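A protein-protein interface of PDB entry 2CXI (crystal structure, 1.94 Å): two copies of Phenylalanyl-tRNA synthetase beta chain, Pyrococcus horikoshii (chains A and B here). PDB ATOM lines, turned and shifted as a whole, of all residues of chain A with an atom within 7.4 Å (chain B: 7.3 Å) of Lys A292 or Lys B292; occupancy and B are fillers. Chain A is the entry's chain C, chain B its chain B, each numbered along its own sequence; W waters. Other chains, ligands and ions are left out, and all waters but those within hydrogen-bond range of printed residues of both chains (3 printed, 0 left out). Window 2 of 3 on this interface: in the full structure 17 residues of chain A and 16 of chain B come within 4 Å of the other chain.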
ATOM      1  N   GLU A 286     -13.155  15.193  22.544  1.00  0.00           N
ATOM      2  CA  GLU A 286     -13.144  16.294  23.507  1.00  0.00           C
ATOM      3  C   GLU A 286     -14.433  17.094  23.380  1.00  0.00           C
ATOM      4  O   GLU A 286     -14.818  17.486  22.270  1.00  0.00           O
ATOM      5  CB  GLU A 286     -11.944  17.241  23.265  1.00  0.00           C
ATOM      6  CG  GLU A 286     -10.593  16.624  23.586  1.00  0.00           C
ATOM      7  CD  GLU A 286     -10.395  16.295  25.072  1.00  0.00           C
ATOM      8  OE1 GLU A 286     -11.099  16.874  25.947  1.00  0.00           O
ATOM      9  OE2 GLU A 286      -9.512  15.464  25.374  1.00  0.00           O
ATOM     10  N   LEU A 287     -15.115  17.353  24.488  1.00  0.00           N
ATOM     11  CA  LEU A 287     -16.344  18.122  24.385  1.00  0.00           C
ATOM     12  C   LEU A 287     -16.076  19.565  23.969  1.00  0.00           C
ATOM     13  O   LEU A 287     -16.949  20.237  23.368  1.00  0.00           O
ATOM     14  CB  LEU A 287     -17.204  17.967  25.650  1.00  0.00           C
ATOM     15  CG  LEU A 287     -17.687  16.501  25.822  1.00  0.00           C
ATOM     16  CD1 LEU A 287     -18.399  16.291  27.110  1.00  0.00           C
ATOM     17  CD2 LEU A 287     -18.555  16.047  24.686  1.00  0.00           C
ATOM     18  N   ASP A 288     -14.859  20.045  24.254  1.00  0.00           N
ATOM     19  CA  ASP A 288     -14.479  21.392  23.841  1.00  0.00           C
ATOM     20  C   ASP A 288     -14.397  21.437  22.318  1.00  0.00           C
ATOM     21  O   ASP A 288     -14.761  22.429  21.723  1.00  0.00           O
ATOM     22  CB  ASP A 288     -13.122  21.817  24.416  1.00  0.00           C
ATOM     23  CG  ASP A 288     -13.201  22.312  25.873  1.00  0.00           C
ATOM     24  OD1 ASP A 288     -14.292  22.355  26.497  1.00  0.00           O
ATOM     25  OD2 ASP A 288     -12.179  22.669  26.487  1.00  0.00           O
ATOM     26  N   TYR A 289     -13.905  20.363  21.700  1.00  0.00           N
ATOM     27  CA  TYR A 289     -13.936  20.228  20.214  1.00  0.00           C
ATOM     28  C   TYR A 289     -15.370  20.395  19.668  1.00  0.00           C
ATOM     29  O   TYR A 289     -15.599  21.135  18.707  1.00  0.00           O
ATOM     30  CB  TYR A 289     -13.299  18.890  19.758  1.00  0.00           C
ATOM     31  CG  TYR A 289     -13.514  18.595  18.287  1.00  0.00           C
ATOM     32  CD1 TYR A 289     -14.671  17.940  17.841  1.00  0.00           C
ATOM     33  CD2 TYR A 289     -12.566  18.977  17.338  1.00  0.00           C
ATOM     34  CE1 TYR A 289     -14.898  17.703  16.466  1.00  0.00           C
ATOM     35  CE2 TYR A 289     -12.767  18.731  15.961  1.00  0.00           C
ATOM     36  CZ  TYR A 289     -13.937  18.096  15.542  1.00  0.00           C
ATOM     37  OH  TYR A 289     -14.144  17.866  14.201  1.00  0.00           O
ATOM     38  N   ILE A 290     -16.333  19.718  20.279  1.00  0.00           N
ATOM     39  CA  ILE A 290     -17.756  19.878  19.903  1.00  0.00           C
ATOM     40  C   ILE A 290     -18.259  21.328  20.020  1.00  0.00           C
ATOM     41  O   ILE A 290     -18.854  21.857  19.083  1.00  0.00           O
ATOM     42  CB  ILE A 290     -18.676  18.923  20.693  1.00  0.00           C
ATOM     43  CG1 ILE A 290     -18.227  17.450  20.557  1.00  0.00           C
ATOM     44  CG2 ILE A 290     -20.172  19.119  20.269  1.00  0.00           C
ATOM     45  CD1 ILE A 290     -18.390  16.839  19.099  1.00  0.00           C
ATOM     46  N   ARG A 291     -18.007  21.982  21.154  1.00  0.00           N
ATOM     47  CA  ARG A 291     -18.390  23.387  21.329  1.00  0.00           C
ATOM     48  C   ARG A 291     -17.754  24.316  20.295  1.00  0.00           C
ATOM     49  O   ARG A 291     -18.441  25.148  19.720  1.00  0.00           O
ATOM     50  CB  ARG A 291     -18.043  23.866  22.734  1.00  0.00           C
ATOM     51  CG  ARG A 291     -19.014  23.400  23.808  1.00  0.00           C
ATOM     52  CD  ARG A 291     -18.639  23.882  25.242  1.00  0.00           C
ATOM     53  NE  ARG A 291     -17.656  23.010  25.886  1.00  0.00           N
ATOM     54  CZ  ARG A 291     -17.956  21.895  26.548  1.00  0.00           C
ATOM     55  NH1 ARG A 291     -19.211  21.497  26.661  1.00  0.00           N
ATOM     56  NH2 ARG A 291     -17.000  21.170  27.099  1.00  0.00           N
ATOM     57  N   LYS A 292     -16.453  24.172  20.062  1.00  0.00           N
ATOM     58  CA  LYS A 292     -15.735  25.115  19.205  1.00  0.00           C
ATOM     59  C   LYS A 292     -16.201  24.993  17.766  1.00  0.00           C
ATOM     60  O   LYS A 292     -16.552  26.002  17.125  1.00  0.00           O
ATOM     61  CB  LYS A 292     -14.214  24.892  19.280  1.00  0.00           C
ATOM     62  CG  LYS A 292     -13.339  25.998  18.561  1.00  0.00           C
ATOM     63  CD  LYS A 292     -13.456  27.400  19.263  1.00  0.00           C
ATOM     64  CE  LYS A 292     -12.626  27.485  20.556  1.00  0.00           C
ATOM     65  NZ  LYS A 292     -13.124  28.591  21.474  1.00  0.00           N
ATOM     66  N   LEU A 293     -16.212  23.765  17.243  1.00  0.00           N
ATOM     67  CA  LEU A 293     -16.617  23.573  15.857  1.00  0.00           C
ATOM     68  C   LEU A 293     -18.112  23.762  15.603  1.00  0.00           C
ATOM     69  O   LEU A 293     -18.510  24.152  14.506  1.00  0.00           O
ATOM     70  CB  LEU A 293     -16.163  22.218  15.344  1.00  0.00           C
ATOM     71  CG  LEU A 293     -14.690  21.852  15.081  1.00  0.00           C
ATOM     72  CD1 LEU A 293     -14.407  22.023  13.593  1.00  0.00           C
ATOM     73  CD2 LEU A 293     -13.626  22.528  15.995  1.00  0.00           C
ATOM     74  N   SER A 294     -18.954  23.500  16.594  1.00  0.00           N
ATOM     75  CA  SER A 294     -20.399  23.699  16.392  1.00  0.00           C
ATOM     76  C   SER A 294     -20.804  25.181  16.434  1.00  0.00           C
ATOM     77  O   SER A 294     -21.732  25.592  15.749  1.00  0.00           O
ATOM     78  CB  SER A 294     -21.214  22.918  17.417  1.00  0.00           C
ATOM     79  OG  SER A 294     -20.983  23.421  18.731  1.00  0.00           O
ATOM     80  N   GLY A 295     -20.085  25.960  17.251  1.00  0.00           N
ATOM     81  CA  GLY A 295     -20.444  27.350  17.539  1.00  0.00           C
ATOM     82  C   GLY A 295     -21.592  27.388  18.528  1.00  0.00           C
ATOM     83  O   GLY A 295     -22.252  28.409  18.696  1.00  0.00           O
ATOM     84  N   LEU A 296     -21.867  26.253  19.164  1.00  0.00           N
ATOM     85  CA  LEU A 296     -22.949  26.186  20.105  1.00  0.00           C
ATOM     86  C   LEU A 296     -22.339  26.068  21.487  1.00  0.00           C
ATOM     87  O   LEU A 296     -21.490  25.209  21.728  1.00  0.00           O
ATOM     88  CB  LEU A 296     -23.859  24.992  19.816  1.00  0.00           C
ATOM     89  CG  LEU A 296     -24.691  24.983  18.535  1.00  0.00           C
ATOM     90  CD1 LEU A 296     -25.269  23.590  18.389  1.00  0.00           C
ATOM     91  CD2 LEU A 296     -25.818  26.019  18.587  1.00  0.00           C
ATOM     92  N   GLU A 297     -22.756  26.935  22.392  1.00  0.00           N
ATOM     93  CA  GLU A 297     -22.319  26.778  23.765  1.00  0.00           C
ATOM     94  C   GLU A 297     -23.282  25.808  24.460  1.00  0.00           C
ATOM     95  O   GLU A 297     -24.290  26.188  25.089  1.00  0.00           O
ATOM     96  CB  GLU A 297     -22.137  28.133  24.477  1.00  0.00           C
ATOM     97  CG  GLU A 297     -20.730  28.715  24.304  1.00  0.00           C
ATOM     98  CD  GLU A 297     -19.631  27.826  24.897  1.00  0.00           C
ATOM     99  OE1 GLU A 297     -19.796  27.359  26.055  1.00  0.00           O
ATOM    100  OE2 GLU A 297     -18.599  27.584  24.215  1.00  0.00           O
ATOM    101  N   LEU A 339     -19.361  15.377  15.839  1.00  0.00           N
ATOM    102  CA  LEU A 339     -19.914  16.707  15.652  1.00  0.00           C
ATOM    103  C   LEU A 339     -21.155  16.742  14.741  1.00  0.00           C
ATOM    104  O   LEU A 339     -22.158  17.366  15.086  1.00  0.00           O
ATOM    105  CB  LEU A 339     -18.838  17.661  15.116  1.00  0.00           C
ATOM    106  CG  LEU A 339     -19.306  19.005  14.534  1.00  0.00           C
ATOM    107  CD1 LEU A 339     -19.801  19.955  15.632  1.00  0.00           C
ATOM    108  CD2 LEU A 339     -18.156  19.631  13.738  1.00  0.00           C
ATOM    109  N   LEU B 287     -17.898  36.371  16.034  1.00  0.00           N
ATOM    110  CA  LEU B 287     -16.960  36.549  14.925  1.00  0.00           C
ATOM    111  C   LEU B 287     -15.682  35.739  15.088  1.00  0.00           C
ATOM    112  O   LEU B 287     -15.063  35.349  14.088  1.00  0.00           O
ATOM    113  CB  LEU B 287     -16.693  38.041  14.658  1.00  0.00           C
ATOM    114  CG  LEU B 287     -17.982  38.812  14.258  1.00  0.00           C
ATOM    115  CD1 LEU B 287     -17.774  40.318  14.245  1.00  0.00           C
ATOM    116  CD2 LEU B 287     -18.483  38.398  12.896  1.00  0.00           C
ATOM    117  N   ASP B 288     -15.276  35.461  16.336  1.00  0.00           N
ATOM    118  CA  ASP B 288     -14.175  34.512  16.543  1.00  0.00           C
ATOM    119  C   ASP B 288     -14.394  33.166  15.848  1.00  0.00           C
ATOM    120  O   ASP B 288     -13.427  32.525  15.416  1.00  0.00           O
ATOM    121  CB  ASP B 288     -13.963  34.217  18.009  1.00  0.00           C
ATOM    122  CG  ASP B 288     -13.363  35.383  18.747  1.00  0.00           C
ATOM    123  OD1 ASP B 288     -12.908  36.393  18.135  1.00  0.00           O
ATOM    124  OD2 ASP B 288     -13.335  35.339  19.969  1.00  0.00           O
ATOM    125  N   TYR B 289     -15.645  32.723  15.823  1.00  0.00           N
ATOM    126  CA  TYR B 289     -16.017  31.469  15.130  1.00  0.00           C
ATOM    127  C   TYR B 289     -15.625  31.494  13.629  1.00  0.00           C
ATOM    128  O   TYR B 289     -15.021  30.555  13.125  1.00  0.00           O
ATOM    129  CB  TYR B 289     -17.524  31.195  15.274  1.00  0.00           C
ATOM    130  CG  TYR B 289     -17.974  29.944  14.536  1.00  0.00           C
ATOM    131  CD1 TYR B 289     -18.437  30.016  13.209  1.00  0.00           C
ATOM    132  CD2 TYR B 289     -17.902  28.697  15.148  1.00  0.00           C
ATOM    133  CE1 TYR B 289     -18.839  28.872  12.530  1.00  0.00           C
ATOM    134  CE2 TYR B 289     -18.321  27.531  14.468  1.00  0.00           C
ATOM    135  CZ  TYR B 289     -18.798  27.642  13.171  1.00  0.00           C
ATOM    136  OH  TYR B 289     -19.190  26.505  12.497  1.00  0.00           O
ATOM    137  N   ILE B 290     -15.954  32.583  12.952  1.00  0.00           N
ATOM    138  CA  ILE B 290     -15.619  32.789  11.564  1.00  0.00           C
ATOM    139  C   ILE B 290     -14.089  32.696  11.322  1.00  0.00           C
ATOM    140  O   ILE B 290     -13.635  31.981  10.418  1.00  0.00           O
ATOM    141  CB  ILE B 290     -16.249  34.145  11.009  1.00  0.00           C
ATOM    142  CG1 ILE B 290     -17.804  34.197  11.158  1.00  0.00           C
ATOM    143  CG2 ILE B 290     -15.802  34.384   9.555  1.00  0.00           C
ATOM    144  CD1 ILE B 290     -18.636  33.048  10.401  1.00  0.00           C
ATOM    145  N   ARG B 291     -13.312  33.410  12.139  1.00  0.00           N
ATOM    146  CA  ARG B 291     -11.839  33.312  12.101  1.00  0.00           C
ATOM    147  C   ARG B 291     -11.342  31.891  12.370  1.00  0.00           C
ATOM    148  O   ARG B 291     -10.548  31.375  11.594  1.00  0.00           O
ATOM    149  CB  ARG B 291     -11.185  34.289  13.102  1.00  0.00           C
ATOM    150  CG  ARG B 291     -11.153  35.783  12.647  1.00  0.00           C
ATOM    151  CD  ARG B 291     -10.512  36.756  13.678  1.00  0.00           C
ATOM    152  NE  ARG B 291     -11.457  37.021  14.766  1.00  0.00           N
ATOM    153  CZ  ARG B 291     -12.408  37.942  14.742  1.00  0.00           C
ATOM    154  NH1 ARG B 291     -12.553  38.747  13.687  1.00  0.00           N
ATOM    155  NH2 ARG B 291     -13.240  38.047  15.773  1.00  0.00           N
ATOM    156  N   LYS B 292     -11.823  31.264  13.443  1.00  0.00           N
ATOM    157  CA  LYS B 292     -11.346  29.940  13.873  1.00  0.00           C
ATOM    158  C   LYS B 292     -11.488  28.928  12.714  1.00  0.00           C
ATOM    159  O   LYS B 292     -10.522  28.290  12.313  1.00  0.00           O
ATOM    160  CB  LYS B 292     -12.176  29.447  15.079  1.00  0.00           C
ATOM    161  CG  LYS B 292     -11.678  28.156  15.787  1.00  0.00           C
ATOM    162  CD  LYS B 292     -10.601  28.504  16.869  1.00  0.00           C
ATOM    163  CE  LYS B 292      -9.823  27.300  17.343  1.00  0.00           C
ATOM    164  NZ  LYS B 292      -8.553  27.800  17.964  1.00  0.00           N
ATOM    165  N   LEU B 293     -12.705  28.816  12.195  1.00  0.00           N
ATOM    166  CA  LEU B 293     -13.064  27.775  11.223  1.00  0.00           C
ATOM    167  C   LEU B 293     -12.576  28.106   9.811  1.00  0.00           C
ATOM    168  O   LEU B 293     -12.224  27.194   9.057  1.00  0.00           O
ATOM    169  CB  LEU B 293     -14.581  27.573  11.233  1.00  0.00           C
ATOM    170  CG  LEU B 293     -15.274  26.628  12.216  1.00  0.00           C
ATOM    171  CD1 LEU B 293     -15.179  25.221  11.748  1.00  0.00           C
ATOM    172  CD2 LEU B 293     -14.787  26.742  13.674  1.00  0.00           C
ATOM    173  N   SER B 294     -12.531  29.390   9.444  1.00  0.00           N
ATOM    174  CA  SER B 294     -12.020  29.775   8.106  1.00  0.00           C
ATOM    175  C   SER B 294     -10.509  29.618   8.015  1.00  0.00           C
ATOM    176  O   SER B 294      -9.973  29.354   6.939  1.00  0.00           O
ATOM    177  CB  SER B 294     -12.381  31.217   7.741  1.00  0.00           C
ATOM    178  OG  SER B 294     -11.701  32.161   8.573  1.00  0.00           O
ATOM    179  N   GLY B 295      -9.844  29.825   9.151  1.00  0.00           N
ATOM    180  CA  GLY B 295      -8.395  29.886   9.233  1.00  0.00           C
ATOM    181  C   GLY B 295      -7.865  31.229   8.773  1.00  0.00           C
ATOM    182  O   GLY B 295      -6.644  31.392   8.630  1.00  0.00           O
ATOM    183  N   LEU B 296      -8.764  32.181   8.536  1.00  0.00           N
ATOM    184  CA  LEU B 296      -8.388  33.522   8.135  1.00  0.00           C
ATOM    185  C   LEU B 296      -8.406  34.409   9.371  1.00  0.00           C
ATOM    186  O   LEU B 296      -9.197  34.150  10.298  1.00  0.00           O
ATOM    187  CB  LEU B 296      -9.361  34.063   7.085  1.00  0.00           C
ATOM    188  CG  LEU B 296      -9.518  33.204   5.816  1.00  0.00           C
ATOM    189  CD1 LEU B 296     -10.729  33.603   4.954  1.00  0.00           C
ATOM    190  CD2 LEU B 296      -8.251  33.290   5.004  1.00  0.00           C
ATOM    191  N   GLU B 297      -7.565  35.450   9.394  1.00  0.00           N
ATOM    192  CA  GLU B 297      -7.585  36.390  10.523  1.00  0.00           C
ATOM    193  C   GLU B 297      -8.275  37.698  10.162  1.00  0.00           C
ATOM    194  O   GLU B 297      -7.850  38.771  10.601  1.00  0.00           O
ATOM    195  CB  GLU B 297      -6.167  36.617  11.103  1.00  0.00           C
ATOM    196  CG  GLU B 297      -5.490  35.344  11.584  1.00  0.00           C
ATOM    197  CD  GLU B 297      -6.154  34.729  12.811  1.00  0.00           C
ATOM    198  OE1 GLU B 297      -6.851  35.434  13.559  1.00  0.00           O
ATOM    199  OE2 GLU B 297      -5.948  33.536  13.049  1.00  0.00           O
ATOM    200  N   ALA B 335     -24.144  27.786  12.693  1.00  0.00           N
ATOM    201  CA  ALA B 335     -23.075  28.778  12.536  1.00  0.00           C
ATOM    202  C   ALA B 335     -22.245  28.521  11.284  1.00  0.00           C
ATOM    203  O   ALA B 335     -21.818  29.449  10.628  1.00  0.00           O
ATOM    204  CB  ALA B 335     -22.174  28.824  13.792  1.00  0.00           C
ATOM    205  N   LEU B 339     -20.513  30.901   8.132  1.00  0.00           N
ATOM    206  CA  LEU B 339     -19.141  30.673   7.675  1.00  0.00           C
ATOM    207  C   LEU B 339     -19.108  30.402   6.168  1.00  0.00           C
ATOM    208  O   LEU B 339     -18.310  30.962   5.440  1.00  0.00           O
ATOM    209  CB  LEU B 339     -18.505  29.489   8.448  1.00  0.00           C
ATOM    210  CG  LEU B 339     -17.182  28.904   7.918  1.00  0.00           C
ATOM    211  CD1 LEU B 339     -16.060  29.931   8.012  1.00  0.00           C
ATOM    212  CD2 LEU B 339     -16.815  27.631   8.638  1.00  0.00           C
HETATM  213  O   HOH W   1     -22.053  25.048  12.986  1.00  0.00           O
HETATM  214  O   HOH W   2     -24.349  26.530  15.345  1.00  0.00           O
HETATM  215  O   HOH W   3     -20.066  23.259  12.625  1.00  0.00           O
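Lys A292 touches Tyr B289, but with the chains exchanged Tyr A289 does not touch Lys B292 (8.6 Å). Lys A292 touches its own counterpart, Lys B292. Leu A293 touches Tyr B289, but with the chains exchanged Tyr A289 does not touch Leu B293 (7.6 Å). Ser A294 touches Tyr B289, but with the chains exchanged Tyr A289 does not touch Ser B294 (12.5 Å). Positions printed for both chains: 287, 288, 289, 290, 291, 292, 293, 294, 295, 296, 297 and 339.
Of chain B, only Tyr B289 (3.5 Å), Lys B292 (3.9 Å) and Leu B293 (3.9 Å) come within 4 Å of Lys A292. Lys B292 touches just one residue of chain A: Lys A292. Of the printed residues of chain B, Leu A293 touches Tyr B289 and Leu B293. Of the printed residues of chain A, Ala B335 touches Ser A294. Of the printed residues of chain B, Ser A294 touches Tyr B289 (3.9 Å) and Ala B335 (3.8 Å). Of the printed residues of chain B, Gly A295 touches Tyr B289 (3.7 Å). Of the printed residues of chain A, Tyr B289 touches Lys A292, Leu A293, Ser A294 and Gly A295.
Printed residues of chain A that touch a printed residue of chain B: Lys A292, Leu A293, Ser A294 and Gly A295. Hydrophobic or aromatic side chains of chain A that line the printed part of chain B: Leu A293. Along chain A the printed residues that touch a printed residue of chain B span positions 292 to 295. Of the 13 printed residues of chain B, 4 touch a printed residue of chain A. Hydrophobic or aromatic side chains of chain B within 4 Å of the printed part of chain A: Tyr B289, Leu B293 and Ala B335. Along chain B the printed residues that touch a printed residue of chain A span positions 289 to 335.
N of Leu A296 is in hydrogen-bond range of OG of Ser A294 (3.0 Å). The side-chain hydroxyl of Ser A294 sits at hydrogen-bond distance from the backbone carbonyl oxygen of Ile A290 (2.7 Å). O of Arg A291 is in hydrogen-bond range of OG of Ser A294 (3.2 Å).
Lys A292 touches Tyr B289 (O to CE2, 3.5 Å). CD of Lys B292 touches CD of Lys A292 (3.9 Å). Leu B293 touches Lys A292. CD1 of Leu A293 touches CD1 of Leu B293, at 3.8 Å. Ser A294 touches Tyr B289. Ser A294 touches Ala B335 (O to CB, 3.8 Å). Tyr B289 touches Gly A295.
The side-chain hydroxyl (OH) of Tyr B289 sits at hydrogen-bond distance from the backbone carbonyl oxygen (O) of Leu A293 (3.2 Å).
Water W3 bridges the backbone carbonyl oxygen of Leu A293 (2.6 Å) and the side-chain hydroxyl of Tyr B289 (3.4 Å). Water W2 lies within hydrogen-bond range of the backbone carbonyl oxygen of Ser A294 and the backbone NH of Ala B335. Water W1 lies within hydrogen-bond range of the backbone carbonyl oxygen of Ser A294, the side-chain hydroxyl of Tyr B289 and the backbone NH of Ala B335.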
